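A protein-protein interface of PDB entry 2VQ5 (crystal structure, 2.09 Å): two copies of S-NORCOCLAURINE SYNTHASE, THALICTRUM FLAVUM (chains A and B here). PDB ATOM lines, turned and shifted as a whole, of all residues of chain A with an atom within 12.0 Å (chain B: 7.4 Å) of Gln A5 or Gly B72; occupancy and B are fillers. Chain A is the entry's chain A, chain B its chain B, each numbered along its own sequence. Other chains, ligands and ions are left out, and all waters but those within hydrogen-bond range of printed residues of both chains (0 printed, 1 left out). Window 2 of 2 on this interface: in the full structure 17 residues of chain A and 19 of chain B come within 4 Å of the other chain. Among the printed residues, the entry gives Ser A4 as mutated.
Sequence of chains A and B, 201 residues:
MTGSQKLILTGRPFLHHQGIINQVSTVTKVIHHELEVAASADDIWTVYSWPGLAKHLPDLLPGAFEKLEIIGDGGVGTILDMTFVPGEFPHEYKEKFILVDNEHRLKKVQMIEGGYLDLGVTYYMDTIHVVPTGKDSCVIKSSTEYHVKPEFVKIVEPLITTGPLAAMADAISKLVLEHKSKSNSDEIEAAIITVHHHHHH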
ATOM      1  N   SER A   4      12.742 -14.843 -14.836  1.00  0.00           N
ATOM      2  CA  SER A   4      14.243 -14.807 -14.824  1.00  0.00           C
ATOM      3  C   SER A   4      14.803 -13.488 -14.277  1.00  0.00           C
ATOM      4  O   SER A   4      14.060 -12.525 -14.046  1.00  0.00           O
ATOM      5  CB  SER A   4      14.812 -15.084 -16.222  1.00  0.00           C
ATOM      6  OG  SER A   4      14.266 -14.187 -17.176  1.00  0.00           O
ATOM      7  N   GLN A   5      16.126 -13.471 -14.096  1.00  0.00           N
ATOM      8  CA  GLN A   5      16.839 -12.373 -13.445  1.00  0.00           C
ATOM      9  C   GLN A   5      16.748 -11.025 -14.181  1.00  0.00           C
ATOM     10  O   GLN A   5      16.910 -10.949 -15.399  1.00  0.00           O
ATOM     11  CB  GLN A   5      18.303 -12.761 -13.197  1.00  0.00           C
ATOM     12  CG  GLN A   5      18.467 -13.997 -12.305  1.00  0.00           C
ATOM     13  CD  GLN A   5      19.807 -14.047 -11.579  1.00  0.00           C
ATOM     14  OE1 GLN A   5      20.860 -13.725 -12.154  1.00  0.00           O
ATOM     15  NE2 GLN A   5      19.775 -14.466 -10.311  1.00  0.00           N
ATOM     16  N   LYS A   6      16.456  -9.976 -13.414  1.00  0.00           N
ATOM     17  CA  LYS A   6      16.403  -8.620 -13.944  1.00  0.00           C
ATOM     18  C   LYS A   6      17.453  -7.758 -13.254  1.00  0.00           C
ATOM     19  O   LYS A   6      17.432  -7.554 -12.026  1.00  0.00           O
ATOM     20  CB  LYS A   6      15.014  -8.013 -13.798  1.00  0.00           C
ATOM     21  CG  LYS A   6      13.911  -8.743 -14.537  1.00  0.00           C
ATOM     22  CD  LYS A   6      12.638  -7.904 -14.562  1.00  0.00           C
ATOM     23  CE  LYS A   6      11.438  -8.683 -15.093  1.00  0.00           C
ATOM     24  NZ  LYS A   6      10.239  -7.793 -15.253  1.00  0.00           N
ATOM     25  N   LEU A   7      18.390  -7.275 -14.049  1.00  0.00           N
ATOM     26  CA  LEU A   7      19.438  -6.419 -13.538  1.00  0.00           C
ATOM     27  C   LEU A   7      19.375  -5.094 -14.275  1.00  0.00           C
ATOM     28  O   LEU A   7      19.402  -5.064 -15.506  1.00  0.00           O
ATOM     29  CB  LEU A   7      20.807  -7.094 -13.710  1.00  0.00           C
ATOM     30  CG  LEU A   7      22.053  -6.278 -13.368  1.00  0.00           C
ATOM     31  CD1 LEU A   7      22.284  -6.229 -11.856  1.00  0.00           C
ATOM     32  CD2 LEU A   7      23.280  -6.832 -14.084  1.00  0.00           C
ATOM     33  N   ILE A   8      19.296  -4.002 -13.515  1.00  0.00           N
ATOM     34  CA  ILE A   8      19.250  -2.652 -14.075  1.00  0.00           C
ATOM     35  C   ILE A   8      20.509  -1.867 -13.691  1.00  0.00           C
ATOM     36  O   ILE A   8      20.852  -1.731 -12.513  1.00  0.00           O
ATOM     37  CB  ILE A   8      17.961  -1.901 -13.647  1.00  0.00           C
ATOM     38  CG1 ILE A   8      16.724  -2.755 -13.967  1.00  0.00           C
ATOM     39  CG2 ILE A   8      17.883  -0.513 -14.308  1.00  0.00           C
ATOM     40  CD1 ILE A   8      15.450  -2.328 -13.264  1.00  0.00           C
ATOM     41  N   LEU A   9      21.209  -1.368 -14.701  1.00  0.00           N
ATOM     42  CA  LEU A   9      22.417  -0.602 -14.471  1.00  0.00           C
ATOM     43  C   LEU A   9      22.192   0.843 -14.893  1.00  0.00           C
ATOM     44  O   LEU A   9      21.962   1.146 -16.070  1.00  0.00           O
ATOM     45  CB  LEU A   9      23.607  -1.237 -15.195  1.00  0.00           C
ATOM     46  CG  LEU A   9      23.846  -2.735 -14.925  1.00  0.00           C
ATOM     47  CD1 LEU A   9      24.797  -3.319 -15.967  1.00  0.00           C
ATOM     48  CD2 LEU A   9      24.359  -3.016 -13.510  1.00  0.00           C
ATOM     49  N   PRO B  51      28.585 -14.392 -22.667  1.00  0.00           N
ATOM     50  CA  PRO B  51      27.317 -14.066 -21.995  1.00  0.00           C
ATOM     51  C   PRO B  51      27.447 -12.904 -20.994  1.00  0.00           C
ATOM     52  O   PRO B  51      26.470 -12.193 -20.748  1.00  0.00           O
ATOM     53  CB  PRO B  51      26.937 -15.375 -21.280  1.00  0.00           C
ATOM     54  CG  PRO B  51      27.743 -16.440 -21.947  1.00  0.00           C
ATOM     55  CD  PRO B  51      29.004 -15.784 -22.415  1.00  0.00           C
ATOM     56  N   ALA B  54      26.722  -8.397 -21.779  1.00  0.00           N
ATOM     57  CA  ALA B  54      25.564  -7.528 -21.571  1.00  0.00           C
ATOM     58  C   ALA B  54      25.756  -6.653 -20.339  1.00  0.00           C
ATOM     59  O   ALA B  54      25.602  -5.428 -20.411  1.00  0.00           O
ATOM     60  CB  ALA B  54      24.287  -8.351 -21.453  1.00  0.00           C
ATOM     61  N   LYS B  55      26.121  -7.277 -19.218  1.00  0.00           N
ATOM     62  CA  LYS B  55      26.300  -6.545 -17.959  1.00  0.00           C
ATOM     63  C   LYS B  55      27.513  -5.603 -17.981  1.00  0.00           C
ATOM     64  O   LYS B  55      27.686  -4.780 -17.085  1.00  0.00           O
ATOM     65  CB  LYS B  55      26.333  -7.498 -16.746  1.00  0.00           C
ATOM     66  CG  LYS B  55      27.641  -8.259 -16.570  1.00  0.00           C
ATOM     67  CD  LYS B  55      27.616  -9.158 -15.333  1.00  0.00           C
ATOM     68  CE  LYS B  55      26.927 -10.491 -15.635  1.00  0.00           C
ATOM     69  NZ  LYS B  55      26.784 -11.280 -14.397  1.00  0.00           N
ATOM     70  N   GLU B  69      18.553  -2.242 -18.668  1.00  0.00           N
ATOM     71  CA  GLU B  69      18.038  -3.398 -17.955  1.00  0.00           C
ATOM     72  C   GLU B  69      18.356  -4.682 -18.715  1.00  0.00           C
ATOM     73  O   GLU B  69      18.062  -4.795 -19.903  1.00  0.00           O
ATOM     74  CB  GLU B  69      16.541  -3.282 -17.683  1.00  0.00           C
ATOM     75  CG  GLU B  69      15.974  -4.483 -16.916  1.00  0.00           C
ATOM     76  CD  GLU B  69      14.478  -4.385 -16.684  1.00  0.00           C
ATOM     77  OE1 GLU B  69      13.828  -3.503 -17.279  1.00  0.00           O
ATOM     78  OE2 GLU B  69      13.945  -5.188 -15.890  1.00  0.00           O
ATOM     79  N   ILE B  70      18.970  -5.631 -18.012  1.00  0.00           N
ATOM     80  CA  ILE B  70      19.258  -6.952 -18.551  1.00  0.00           C
ATOM     81  C   ILE B  70      18.303  -7.988 -17.971  1.00  0.00           C
ATOM     82  O   ILE B  70      18.253  -8.212 -16.747  1.00  0.00           O
ATOM     83  CB  ILE B  70      20.711  -7.361 -18.276  1.00  0.00           C
ATOM     84  CG1 ILE B  70      21.645  -6.296 -18.868  1.00  0.00           C
ATOM     85  CG2 ILE B  70      20.997  -8.764 -18.850  1.00  0.00           C
ATOM     86  CD1 ILE B  70      22.655  -5.779 -17.911  1.00  0.00           C
ATOM     87  N   ILE B  71      17.539  -8.604 -18.863  1.00  0.00           N
ATOM     88  CA  ILE B  71      16.575  -9.613 -18.490  1.00  0.00           C
ATOM     89  C   ILE B  71      17.111 -10.952 -19.020  1.00  0.00           C
ATOM     90  O   ILE B  71      16.985 -11.257 -20.207  1.00  0.00           O
ATOM     91  CB  ILE B  71      15.176  -9.268 -19.052  1.00  0.00           C
ATOM     92  CG1 ILE B  71      14.767  -7.837 -18.642  1.00  0.00           C
ATOM     93  CG2 ILE B  71      14.132 -10.272 -18.598  1.00  0.00           C
ATOM     94  CD1 ILE B  71      13.716  -7.181 -19.565  1.00  0.00           C
ATOM     95  N   GLY B  72      17.744 -11.723 -18.136  1.00  0.00           N
ATOM     96  CA  GLY B  72      18.320 -13.018 -18.510  1.00  0.00           C
ATOM     97  C   GLY B  72      19.787 -13.132 -18.163  1.00  0.00           C
ATOM     98  O   GLY B  72      20.376 -12.205 -17.584  1.00  0.00           O
ATOM     99  N   ASP B  73      20.391 -14.260 -18.542  1.00  0.00           N
ATOM    100  CA  ASP B  73      21.779 -14.594 -18.168  1.00  0.00           C
ATOM    101  C   ASP B  73      22.845 -14.003 -19.105  1.00  0.00           C
ATOM    102  O   ASP B  73      24.049 -14.186 -18.888  1.00  0.00           O
ATOM    103  CB  ASP B  73      21.940 -16.121 -18.072  1.00  0.00           C
ATOM    104  CG  ASP B  73      21.487 -16.847 -19.349  1.00  0.00           C
ATOM    105  OD1 ASP B  73      21.673 -16.307 -20.462  1.00  0.00           O
ATOM    106  OD2 ASP B  73      20.932 -17.963 -19.242  1.00  0.00           O
ATOM    107  N   GLY B  74      22.413 -13.289 -20.145  1.00  0.00           N
ATOM    108  CA  GLY B  74      23.349 -12.682 -21.100  1.00  0.00           C
ATOM    109  C   GLY B  74      23.493 -13.517 -22.369  1.00  0.00           C
ATOM    110  O   GLY B  74      24.062 -13.068 -23.368  1.00  0.00           O
ATOM    111  N   GLY B  75      22.983 -14.743 -22.326  1.00  0.00           N
ATOM    112  CA  GLY B  75      23.027 -15.607 -23.485  1.00  0.00           C
ATOM    113  C   GLY B  75      21.825 -15.443 -24.390  1.00  0.00           C
ATOM    114  O   GLY B  75      20.979 -14.563 -24.199  1.00  0.00           O
ATOM    115  N   GLY B  77      18.374 -15.492 -25.978  1.00  0.00           N
ATOM    116  CA  GLY B  77      17.097 -15.364 -25.266  1.00  0.00           C
ATOM    117  C   GLY B  77      17.039 -14.139 -24.356  1.00  0.00           C
ATOM    118  O   GLY B  77      15.960 -13.691 -23.995  1.00  0.00           O
ATOM    119  N   THR B  78      18.199 -13.586 -24.007  1.00  0.00           N
ATOM    120  CA  THR B  78      18.280 -12.370 -23.186  1.00  0.00           C
ATOM    121  C   THR B  78      17.613 -11.164 -23.857  1.00  0.00           C
ATOM    122  O   THR B  78      17.786 -10.942 -25.052  1.00  0.00           O
ATOM    123  CB  THR B  78      19.743 -12.029 -22.885  1.00  0.00           C
ATOM    124  OG1 THR B  78      20.322 -13.100 -22.134  1.00  0.00           O
ATOM    125  CG2 THR B  78      19.866 -10.737 -22.082  1.00  0.00           C
ATOM    126  N   ILE B  79      16.853 -10.391 -23.081  1.00  0.00           N
ATOM    127  CA  ILE B  79      16.317  -9.111 -23.558  1.00  0.00           C
ATOM    128  C   ILE B  79      17.056  -7.948 -22.878  1.00  0.00           C
ATOM    129  O   ILE B  79      17.312  -7.997 -21.668  1.00  0.00           O
ATOM    130  CB  ILE B  79      14.779  -9.025 -23.346  1.00  0.00           C
ATOM    131  CG1 ILE B  79      14.073 -10.058 -24.242  1.00  0.00           C
ATOM    132  CG2 ILE B  79      14.251  -7.607 -23.641  1.00  0.00           C
ATOM    133  CD1 ILE B  79      12.615 -10.281 -23.928  1.00  0.00           C
ATOM    134  N   LEU B  80      17.439  -6.934 -23.662  1.00  0.00           N
ATOM    135  CA  LEU B  80      18.014  -5.698 -23.107  1.00  0.00           C
ATOM    136  C   LEU B  80      17.034  -4.556 -23.325  1.00  0.00           C
ATOM    137  O   LEU B  80      16.539  -4.354 -24.426  1.00  0.00           O
ATOM    138  CB  LEU B  80      19.370  -5.351 -23.735  1.00  0.00           C
ATOM    139  CG  LEU B  80      20.479  -6.421 -23.843  1.00  0.00           C
ATOM    140  CD1 LEU B  80      21.693  -5.874 -24.591  1.00  0.00           C
ATOM    141  CD2 LEU B  80      20.914  -6.970 -22.496  1.00  0.00           C
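The backbone carbonyl oxygen of Gln A5 is in hydrogen-bond range of the backbone NH of Gly B72 (3.0 Å).
O of Ile B70 sits close to O of Gln A5 (3.3 Å).
N of Ile B70 sits at hydrogen-bond distance from O of Leu A7 (2.6 Å).
No position is printed for both chains.
Of the 10 pairs that touch across the chains among the printed residues, none has its exchanged pair printed and touching as well.
The backbone NH (N) of Ile B71 is in hydrogen-bond range of the backbone carbonyl oxygen (O) of Ile B79 (2.9 Å).
Among the printed residues, pairs that only touch across the chains: Leu A7 with Glu B69 (3.3 Å), Lys A6 with Glu B69 (3.3 Å), Lys A6 with Ile B70 (3.4 Å), Gln A5 with Ile B71 (3.4 Å), Leu A9 with Lys B55 (3.4 Å), Ile A8 with Glu B69 (3.5 Å) and Leu A9 with Ile B70 (3.8 Å).
Of the 14 printed residues of chain B, 5 touch a printed residue of chain A.
Printed residues of chain B that touch a printed residue of chain A: Lys B55, Glu B69, Ile B70, Ile B71 and Gly B72.
Along chain B the printed residues that touch a printed residue of chain A span positions 55 to 72.
Of the 6 printed residues of chain A, 5 touch a printed residue of chain B.
Hydrophobic or aromatic side chains of chain A within 4 Å of the printed part of chain B: Ile A8 and Leu A9.
Among the printed residues, 10 pairs touch across the chains.
Among the printed residues, no Asp or Glu carboxylate lies within 4 Å of a Lys or Arg side-chain nitrogen of the other chain.
Printed residues of chain B within 4 Å of Gln A5: Ile B70 (3.3 Å), Ile B71 (3.4 Å) and Gly B72 (3.0 Å).
Printed residues of chain B within 4 Å of Lys A6: Glu B69 and Ile B70.
Of the printed residues of chain B, Leu A7 touches Glu B69 and Ile B70.
Of the printed residues of chain B, Ile A8 touches Glu B69 (3.5 Å).
Of the printed residues of chain A, Lys B55 touches Leu A9 (3.4 Å).
Of chain A, only Gln A5, Lys A6, Leu A7 and Leu A9 come within 4 Å of Ile B70.
Of chain A, only Gln A5 comes within 4 Å of Ile B71.
Gly B72 touches just one residue of chain A: Gln A5 (3.0 Å).
Asp B73 touches none of the printed residues of chain A.
No residue of chain A comes within 4 Å of Gly B74.
No residue of chain A comes within 4 Å of Gly B75.
No residue of chain A comes within 4 Å of Gly B77.
No residue of chain A comes within 4 Å of Thr B78.
No residue of chain A comes within 4 Å of Ile B79.
The nearest residue of chain B that does not touch Gln A5 is Asp B73 (5.7 Å).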
